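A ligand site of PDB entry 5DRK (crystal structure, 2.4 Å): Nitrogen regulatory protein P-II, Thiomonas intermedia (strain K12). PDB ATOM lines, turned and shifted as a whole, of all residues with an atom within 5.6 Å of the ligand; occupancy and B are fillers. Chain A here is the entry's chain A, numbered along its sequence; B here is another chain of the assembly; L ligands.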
ATOM      1  N   ILE A  15     -10.442   4.134   6.300  1.00  0.00           N
ATOM      2  CA  ILE A  15      -9.040   4.259   6.003  1.00  0.00           C
ATOM      3  C   ILE A  15      -8.735   5.403   5.053  1.00  0.00           C
ATOM      4  O   ILE A  15      -9.189   5.425   3.965  1.00  0.00           O
ATOM      5  CB  ILE A  15      -8.460   2.938   5.486  1.00  0.00           C
ATOM      6  CG1 ILE A  15      -8.751   1.807   6.451  1.00  0.00           C
ATOM      7  CG2 ILE A  15      -6.974   3.039   5.337  1.00  0.00           C
ATOM      8  CD1 ILE A  15      -8.361   0.442   5.939  1.00  0.00           C
ATOM      9  N   SER A  43       0.488   1.634   6.609  1.00  0.00           N
ATOM     10  CA  SER A  43       1.074   1.532   5.292  1.00  0.00           C
ATOM     11  C   SER A  43       0.025   0.767   4.469  1.00  0.00           C
ATOM     12  O   SER A  43      -0.767   0.086   5.022  1.00  0.00           O
ATOM     13  CB  SER A  43       2.463   0.962   5.343  1.00  0.00           C
ATOM     14  OG  SER A  43       2.431  -0.423   5.361  1.00  0.00           O
ATOM     15  N   GLY A  44      -0.013   0.933   3.155  1.00  0.00           N
ATOM     16  CA  GLY A  44      -1.049   0.364   2.315  1.00  0.00           C
ATOM     17  C   GLY A  44      -0.727   0.372   0.838  1.00  0.00           C
ATOM     18  O   GLY A  44       0.117   1.133   0.360  1.00  0.00           O
ATOM     19  N   LYS A  45      -1.382  -0.479   0.112  1.00  0.00           N
ATOM     20  CA  LYS A  45      -1.217  -0.521  -1.286  1.00  0.00           C
ATOM     21  C   LYS A  45      -2.590  -0.259  -1.822  1.00  0.00           C
ATOM     22  O   LYS A  45      -3.563  -0.820  -1.383  1.00  0.00           O
ATOM     23  CB  LYS A  45      -0.704  -1.876  -1.730  1.00  0.00           C
ATOM     24  CG  LYS A  45      -0.982  -2.183  -3.176  1.00  0.00           C
ATOM     25  CD  LYS A  45      -0.197  -3.367  -3.648  1.00  0.00           C
ATOM     26  CE  LYS A  45      -0.745  -3.871  -4.952  1.00  0.00           C
ATOM     27  NZ  LYS A  45       0.373  -3.761  -5.893  1.00  0.00           N
ATOM     28  N   GLY A  46      -2.661   0.635  -2.776  1.00  0.00           N
ATOM     29  CA  GLY A  46      -3.931   0.974  -3.370  1.00  0.00           C
ATOM     30  C   GLY A  46      -3.792   1.268  -4.832  1.00  0.00           C
ATOM     31  O   GLY A  46      -2.791   0.968  -5.409  1.00  0.00           O
ATOM     32  N   SER A  47      -4.819   1.855  -5.413  1.00  0.00           N
ATOM     33  CA  SER A  47      -4.821   2.189  -6.817  1.00  0.00           C
ATOM     34  C   SER A  47      -3.755   3.233  -7.040  1.00  0.00           C
ATOM     35  O   SER A  47      -3.169   3.307  -8.079  1.00  0.00           O
ATOM     36  CB  SER A  47      -6.158   2.737  -7.198  1.00  0.00           C
ATOM     37  OG  SER A  47      -6.384   3.930  -6.516  1.00  0.00           O
ATOM     38  N   HIS A  48      -3.512   4.016  -6.031  1.00  0.00           N
ATOM     39  CA  HIS A  48      -2.514   5.054  -6.065  1.00  0.00           C
ATOM     40  C   HIS A  48      -1.126   4.467  -5.899  1.00  0.00           C
ATOM     41  O   HIS A  48      -0.145   5.165  -5.926  1.00  0.00           O
ATOM     42  CB  HIS A  48      -2.802   6.009  -4.912  1.00  0.00           C
ATOM     43  N   TYR A  51       2.285   3.363   0.206  1.00  0.00           N
ATOM     44  CA  TYR A  51       2.370   4.246   1.364  1.00  0.00           C
ATOM     45  C   TYR A  51       3.187   3.516   2.422  1.00  0.00           C
ATOM     46  O   TYR A  51       3.394   2.333   2.317  1.00  0.00           O
ATOM     47  CB  TYR A  51       1.016   4.444   2.005  1.00  0.00           C
ATOM     48  CG  TYR A  51       0.056   5.423   1.376  1.00  0.00           C
ATOM     49  CD1 TYR A  51       0.105   6.758   1.694  1.00  0.00           C
ATOM     50  CD2 TYR A  51      -0.940   4.992   0.538  1.00  0.00           C
ATOM     51  CE1 TYR A  51      -0.788   7.632   1.153  1.00  0.00           C
ATOM     52  CE2 TYR A  51      -1.840   5.863   0.001  1.00  0.00           C
ATOM     53  CZ  TYR A  51      -1.747   7.182   0.316  1.00  0.00           C
ATOM     54  OH  TYR A  51      -2.642   8.039  -0.247  1.00  0.00           O
ATOM     55  N   LEU A  63      -1.204   7.302   6.463  1.00  0.00           N
ATOM     56  CA  LEU A  63      -2.566   6.736   6.503  1.00  0.00           C
ATOM     57  C   LEU A  63      -2.990   6.476   7.943  1.00  0.00           C
ATOM     58  O   LEU A  63      -2.148   6.119   8.772  1.00  0.00           O
ATOM     59  CB  LEU A  63      -2.648   5.408   5.732  1.00  0.00           C
ATOM     60  CG  LEU A  63      -2.722   5.367   4.205  1.00  0.00           C
ATOM     61  CD1 LEU A  63      -2.751   3.897   3.749  1.00  0.00           C
ATOM     62  CD2 LEU A  63      -3.931   6.144   3.684  1.00  0.00           C
ATOM     63  N   HIS A  89     -10.560  11.476  -3.259  1.00  0.00           N
ATOM     64  CA  HIS A  89      -9.424  11.129  -2.438  1.00  0.00           C
ATOM     65  C   HIS A  89      -9.339   9.638  -2.200  1.00  0.00           C
ATOM     66  O   HIS A  89     -10.281   8.925  -2.275  1.00  0.00           O
ATOM     67  CB  HIS A  89      -9.456  11.784  -1.076  1.00  0.00           C
ATOM     68  CG  HIS A  89      -9.474  13.270  -1.089  1.00  0.00           C
ATOM     69  ND1 HIS A  89     -10.627  13.993  -1.205  1.00  0.00           N
ATOM     70  CD2 HIS A  89      -8.479  14.165  -0.996  1.00  0.00           C
ATOM     71  CE1 HIS A  89     -10.339  15.274  -1.187  1.00  0.00           C
ATOM     72  NE2 HIS A  89      -9.045  15.397  -1.052  1.00  0.00           N
ATOM     73  N   SER A  90      -8.154   9.215  -1.857  1.00  0.00           N
ATOM     74  CA  SER A  90      -7.845   7.853  -1.550  1.00  0.00           C
ATOM     75  C   SER A  90      -8.571   7.403  -0.329  1.00  0.00           C
ATOM     76  O   SER A  90      -8.832   8.186   0.530  1.00  0.00           O
ATOM     77  CB  SER A  90      -6.378   7.780  -1.229  1.00  0.00           C
ATOM     78  OG  SER A  90      -5.659   7.265  -2.303  1.00  0.00           O
ATOM     79  N   GLY A  91      -8.872   6.124  -0.236  1.00  0.00           N
ATOM     80  CA  GLY A  91      -9.532   5.613   0.934  1.00  0.00           C
ATOM     81  C   GLY A  91     -10.680   4.677   0.756  1.00  0.00           C
ATOM     82  O   GLY A  91     -11.221   4.567  -0.296  1.00  0.00           O
ATOM     83  N   VAL A  92     -11.043   4.001   1.823  1.00  0.00           N
ATOM     84  CA  VAL A  92     -12.092   3.040   1.772  1.00  0.00           C
ATOM     85  C   VAL A  92     -12.841   2.958   3.078  1.00  0.00           C
ATOM     86  O   VAL A  92     -12.283   3.215   4.098  1.00  0.00           O
ATOM     87  CB  VAL A  92     -11.522   1.631   1.468  1.00  0.00           C
ATOM     88  CG1 VAL A  92     -11.045   1.509   0.051  1.00  0.00           C
ATOM     89  CG2 VAL A  92     -10.397   1.267   2.387  1.00  0.00           C
ATOM     90  N   PHE A  94     -15.093   0.123   5.213  1.00  0.00           N
ATOM     91  CA  PHE A  94     -15.642  -1.221   5.391  1.00  0.00           C
ATOM     92  C   PHE A  94     -16.709  -1.216   6.488  1.00  0.00           C
ATOM     93  O   PHE A  94     -16.448  -0.794   7.610  1.00  0.00           O
ATOM     94  CB  PHE A  94     -14.539  -2.219   5.740  1.00  0.00           C
ATOM     95  CG  PHE A  94     -13.345  -2.174   4.825  1.00  0.00           C
ATOM     96  CD1 PHE A  94     -13.493  -1.987   3.470  1.00  0.00           C
ATOM     97  CD2 PHE A  94     -12.065  -2.303   5.345  1.00  0.00           C
ATOM     98  CE1 PHE A  94     -12.378  -1.947   2.634  1.00  0.00           C
ATOM     99  CE2 PHE A  94     -10.951  -2.259   4.533  1.00  0.00           C
ATOM    100  CZ  PHE A  94     -11.101  -2.081   3.167  1.00  0.00           C
ATOM    101  N   VAL B  33      -5.683  -9.495  -5.587  1.00  0.00           N
ATOM    102  CA  VAL B  33      -6.120  -8.545  -4.568  1.00  0.00           C
ATOM    103  C   VAL B  33      -5.695  -7.142  -4.973  1.00  0.00           C
ATOM    104  O   VAL B  33      -4.554  -6.925  -5.396  1.00  0.00           O
ATOM    105  CB  VAL B  33      -5.530  -8.891  -3.191  1.00  0.00           C
ATOM    106  CG1 VAL B  33      -5.998  -7.887  -2.129  1.00  0.00           C
ATOM    107  CG2 VAL B  33      -5.925 -10.301  -2.803  1.00  0.00           C
ATOM    108  N   LYS B  34      -6.580  -6.164  -4.825  1.00  0.00           N
ATOM    109  CA  LYS B  34      -6.309  -4.865  -5.420  1.00  0.00           C
ATOM    110  C   LYS B  34      -5.721  -3.884  -4.424  1.00  0.00           C
ATOM    111  O   LYS B  34      -5.259  -2.822  -4.819  1.00  0.00           O
ATOM    112  CB  LYS B  34      -7.577  -4.294  -6.060  1.00  0.00           C
ATOM    113  CG  LYS B  34      -7.980  -5.048  -7.322  1.00  0.00           C
ATOM    114  CD  LYS B  34      -9.048  -4.322  -8.133  1.00  0.00           C
ATOM    115  CE  LYS B  34      -9.393  -5.123  -9.383  1.00  0.00           C
ATOM    116  NZ  LYS B  34     -10.566  -4.564 -10.088  1.00  0.00           N
ATOM    117  N   GLY B  35      -5.705  -4.247  -3.156  1.00  0.00           N
ATOM    118  CA  GLY B  35      -5.095  -3.393  -2.150  1.00  0.00           C
ATOM    119  C   GLY B  35      -4.991  -4.079  -0.808  1.00  0.00           C
ATOM    120  O   GLY B  35      -5.518  -5.177  -0.607  1.00  0.00           O
ATOM    121  N   TYR B  36      -4.297  -3.425   0.113  1.00  0.00           N
ATOM    122  CA  TYR B  36      -4.202  -3.932   1.473  1.00  0.00           C
ATOM    123  C   TYR B  36      -3.648  -2.857   2.386  1.00  0.00           C
ATOM    124  O   TYR B  36      -3.000  -1.925   1.929  1.00  0.00           O
ATOM    125  CB  TYR B  36      -3.336  -5.212   1.541  1.00  0.00           C
ATOM    126  CG  TYR B  36      -1.941  -5.066   0.961  1.00  0.00           C
ATOM    127  CD1 TYR B  36      -0.925  -4.440   1.662  1.00  0.00           C
ATOM    128  CD2 TYR B  36      -1.656  -5.566  -0.303  1.00  0.00           C
ATOM    129  CE1 TYR B  36       0.349  -4.295   1.116  1.00  0.00           C
ATOM    130  CE2 TYR B  36      -0.386  -5.435  -0.847  1.00  0.00           C
ATOM    131  CZ  TYR B  36       0.598  -4.812  -0.138  1.00  0.00           C
ATOM    132  OH  TYR B  36       1.848  -4.689  -0.682  1.00  0.00           O
ATOM    133  N   THR B  37      -3.913  -3.015   3.667  1.00  0.00           N
ATOM    134  CA  THR B  37      -3.482  -2.053   4.661  1.00  0.00           C
ATOM    135  C   THR B  37      -2.691  -2.800   5.746  1.00  0.00           C
ATOM    136  O   THR B  37      -3.111  -3.868   6.187  1.00  0.00           O
ATOM    137  CB  THR B  37      -4.678  -1.341   5.262  1.00  0.00           C
ATOM    138  OG1 THR B  37      -5.346  -0.610   4.222  1.00  0.00           O
ATOM    139  CG2 THR B  37      -4.238  -0.383   6.378  1.00  0.00           C
ATOM    140  N   ILE B  38      -1.556  -2.265   6.148  1.00  0.00           N
ATOM    141  CA  ILE B  38      -0.706  -2.997   7.084  1.00  0.00           C
ATOM    142  C   ILE B  38      -0.532  -2.245   8.386  1.00  0.00           C
ATOM    143  O   ILE B  38      -0.087  -1.102   8.416  1.00  0.00           O
ATOM    144  CB  ILE B  38       0.677  -3.289   6.472  1.00  0.00           C
ATOM    145  CG1 ILE B  38       0.520  -4.242   5.297  1.00  0.00           C
ATOM    146  CG2 ILE B  38       1.622  -3.857   7.527  1.00  0.00           C
ATOM    147  CD1 ILE B  38       1.797  -4.542   4.538  1.00  0.00           C
ATOM    148  N   ILE B  67      -4.501  -6.146   6.505  1.00  0.00           N
ATOM    149  CA  ILE B  67      -5.931  -6.055   6.266  1.00  0.00           C
ATOM    150  C   ILE B  67      -6.161  -6.078   4.771  1.00  0.00           C
ATOM    151  O   ILE B  67      -5.612  -5.230   4.037  1.00  0.00           O
ATOM    152  CB  ILE B  67      -6.539  -4.754   6.914  1.00  0.00           C
ATOM    153  CG1 ILE B  67      -6.188  -4.686   8.420  1.00  0.00           C
ATOM    154  CG2 ILE B  67      -8.055  -4.666   6.678  1.00  0.00           C
ATOM    155  CD1 ILE B  67      -6.400  -3.279   9.061  1.00  0.00           C
ATOM    156  N   ALA B  68      -6.950  -7.031   4.294  1.00  0.00           N
ATOM    157  CA  ALA B  68      -7.217  -7.115   2.855  1.00  0.00           C
ATOM    158  C   ALA B  68      -8.685  -7.372   2.578  1.00  0.00           C
ATOM    159  O   ALA B  68      -9.213  -8.416   2.919  1.00  0.00           O
ATOM    160  CB  ALA B  68      -6.345  -8.221   2.207  1.00  0.00           C
ATOM    161  N   ALA B  69      -9.345  -6.406   1.950  1.00  0.00           N
ATOM    162  CA  ALA B  69     -10.693  -6.588   1.420  1.00  0.00           C
ATOM    163  C   ALA B  69     -10.615  -7.307   0.077  1.00  0.00           C
ATOM    164  O   ALA B  69      -9.901  -6.885  -0.814  1.00  0.00           O
ATOM    165  CB  ALA B  69     -11.388  -5.232   1.277  1.00  0.00           C
ATOM    166  N   VAL B  70     -11.362  -8.388  -0.068  1.00  0.00           N
ATOM    167  CA  VAL B  70     -11.212  -9.242  -1.233  1.00  0.00           C
ATOM    168  C   VAL B  70     -12.558  -9.874  -1.584  1.00  0.00           C
ATOM    169  O   VAL B  70     -13.359 -10.164  -0.699  1.00  0.00           O
ATOM    170  CB  VAL B  70     -10.160 -10.356  -0.993  1.00  0.00           C
ATOM    171  CG1 VAL B  70      -8.824  -9.754  -0.579  1.00  0.00           C
ATOM    172  CG2 VAL B  70     -10.633 -11.342   0.078  1.00  0.00           C
ATOM    173  N   LYS B 105     -13.799  -1.335  -6.993  1.00  0.00           N
ATOM    174  CA  LYS B 105     -12.545  -0.958  -6.420  1.00  0.00           C
ATOM    175  C   LYS B 105     -11.825  -2.118  -5.804  1.00  0.00           C
ATOM    176  O   LYS B 105     -10.692  -2.044  -5.463  1.00  0.00           O
ATOM    177  CB  LYS B 105     -12.804   0.032  -5.317  1.00  0.00           C
ATOM    178  CG  LYS B 105     -11.886   1.211  -5.292  1.00  0.00           C
ATOM    179  CD  LYS B 105     -12.546   2.357  -4.592  1.00  0.00           C
ATOM    180  CE  LYS B 105     -11.782   2.744  -3.356  1.00  0.00           C
ATOM    181  NZ  LYS B 105     -10.489   3.328  -3.678  1.00  0.00           N
ATOM    182  N   PHE B 106     -12.539  -3.199  -5.668  1.00  0.00           N
ATOM    183  CA  PHE B 106     -11.978  -4.358  -4.951  1.00  0.00           C
ATOM    184  C   PHE B 106     -11.894  -5.611  -5.805  1.00  0.00           C
ATOM    185  O   PHE B 106     -11.152  -6.536  -5.443  1.00  0.00           O
ATOM    186  CB  PHE B 106     -12.827  -4.648  -3.728  1.00  0.00           C
ATOM    187  CG  PHE B 106     -12.926  -3.498  -2.796  1.00  0.00           C
ATOM    188  CD1 PHE B 106     -11.937  -3.272  -1.851  1.00  0.00           C
ATOM    189  CD2 PHE B 106     -13.986  -2.598  -2.895  1.00  0.00           C
ATOM    190  CE1 PHE B 106     -12.014  -2.181  -1.003  1.00  0.00           C
ATOM    191  CE2 PHE B 106     -14.071  -1.511  -2.042  1.00  0.00           C
ATOM    192  CZ  PHE B 106     -13.088  -1.307  -1.105  1.00  0.00           C
HETATM  193  P1  LIG L   1      -6.814   3.780  -2.821  1.00  0.00           P
HETATM  194  O1  LIG L   1      -8.045   4.251  -2.330  1.00  0.00           O
HETATM  195  O2  LIG L   1      -6.900   2.787  -3.841  1.00  0.00           O
HETATM  196  O3  LIG L   1      -5.918   4.859  -3.062  1.00  0.00           O
HETATM  197  O4  LIG L   1      -6.168   3.060  -1.630  1.00  0.00           O
HETATM  198  C1  LIG L   1      -5.740   3.795  -0.521  1.00  0.00           C
HETATM  199  C2  LIG L   1      -5.548   2.971   0.711  1.00  0.00           C
HETATM  200  O5  LIG L   1      -6.696   2.294   1.112  1.00  0.00           O
HETATM  201  C3  LIG L   1      -4.481   1.925   0.551  1.00  0.00           C
HETATM  202  O6  LIG L   1      -3.197   2.398   0.775  1.00  0.00           O
HETATM  203  C4  LIG L   1      -4.883   0.942   1.593  1.00  0.00           C
HETATM  204  O7  LIG L   1      -4.316   1.244   2.850  1.00  0.00           O
HETATM  205  C5  LIG L   1      -6.378   1.050   1.680  1.00  0.00           C
HETATM  206  N1  LIG L   1      -6.979  -0.031   0.898  1.00  0.00           N
HETATM  207  C6  LIG L   1      -7.344   0.086  -0.345  1.00  0.00           C
HETATM  208  N2  LIG L   1      -7.857  -1.013  -0.809  1.00  0.00           N
HETATM  209  C7  LIG L   1      -7.804  -1.898   0.122  1.00  0.00           C
HETATM  210  C8  LIG L   1      -8.187  -3.296   0.250  1.00  0.00           C
HETATM  211  N3  LIG L   1      -8.712  -3.978  -0.735  1.00  0.00           N
HETATM  212  N4  LIG L   1      -7.952  -3.871   1.390  1.00  0.00           N
HETATM  213  C9  LIG L   1      -7.428  -3.233   2.375  1.00  0.00           C
HETATM  214  N5  LIG L   1      -7.073  -1.977   2.331  1.00  0.00           N
HETATM  215  C10 LIG L   1      -7.228  -1.252   1.250  1.00  0.00           C
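Gly 44 touches the ligand (C to O6, 3.2 Å). Gly 46 touches the ligand. His 48 touches the ligand. CD2 of Tyr 51 touches O6 of the ligand, at 3.4 Å. CD1 of Leu 63 touches O7 of the ligand (3.2 Å). CG2 of Val 92 touches N1 of the ligand (3.9 Å). CZ of Phe 94 touches C9 of the ligand (3.9 Å). Tyr 36 of chain B touches the ligand. Ile 67 of chain B touches the ligand (O to C9, 3.2 Å). Ala 68 of chain B touches the ligand. Phe 106 of chain B touches the ligand. Hydrophobic or aromatic side chains that line the ligand: His 48, Tyr 51, Leu 63, Val 92, Phe 94, Ala 69 of chain B and Phe 106 of chain B. Of the 26 residues printed, 19 come within 4 Å of the ligand. Along chain A the residues within 4 Å of the ligand span positions 44 to 94. The nearest printed residue that does not touch the ligand is Ile 15 (4.1 Å).
The side-chain hydroxyl (OG1) of Thr 37 of chain B lies within hydrogen-bond range of an oxygen (O7) of the ligand (2.5 Å). An oxygen (O3) of the ligand lies within hydrogen-bond range of the side-chain hydroxyl (OG) of Ser 90. The backbone NH (N) of Ser 47 lies within hydrogen-bond range of an oxygen (O2) of the ligand, 2.8 Å away. An oxygen (O2) of the ligand lies within hydrogen-bond range of the side-chain hydroxyl (OG) of Ser 47 (3.0 Å). The backbone NH (N) of Gly 91 is in hydrogen-bond range of an oxygen (O1) of the ligand (2.9 Å). NZ of Lys 105 of chain B lies within salt-bridge range of O1 of the ligand. The backbone NH of Ala 69 of chain B is in hydrogen-bond range of a nitrogen (N4) of the ligand (2.9 Å). O of Ala 69 of chain B sits at hydrogen-bond distance from N3 of the ligand, 3.1 Å away. A nitrogen (N3) of the ligand sits close to the backbone carbonyl oxygen (O) of Gly 35 of chain B, at 3.4 Å. The backbone NH (N) of Lys 45 lies within hydrogen-bond range of an oxygen (O6) of the ligand.
The backbone carbonyl oxygen of Thr 37 of chain B sits at hydrogen-bond distance from the backbone NH of Ile 67 of chain B (2.7 Å). The backbone NH (N) of Tyr 51 lies within hydrogen-bond range of the backbone carbonyl oxygen (O) of Gly 44, 3.1 Å away. O of Tyr 36 of chain B is in hydrogen-bond range of N of Lys 45. O of Val 92 is in hydrogen-bond range of N of Ile 15, 3.0 Å away.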
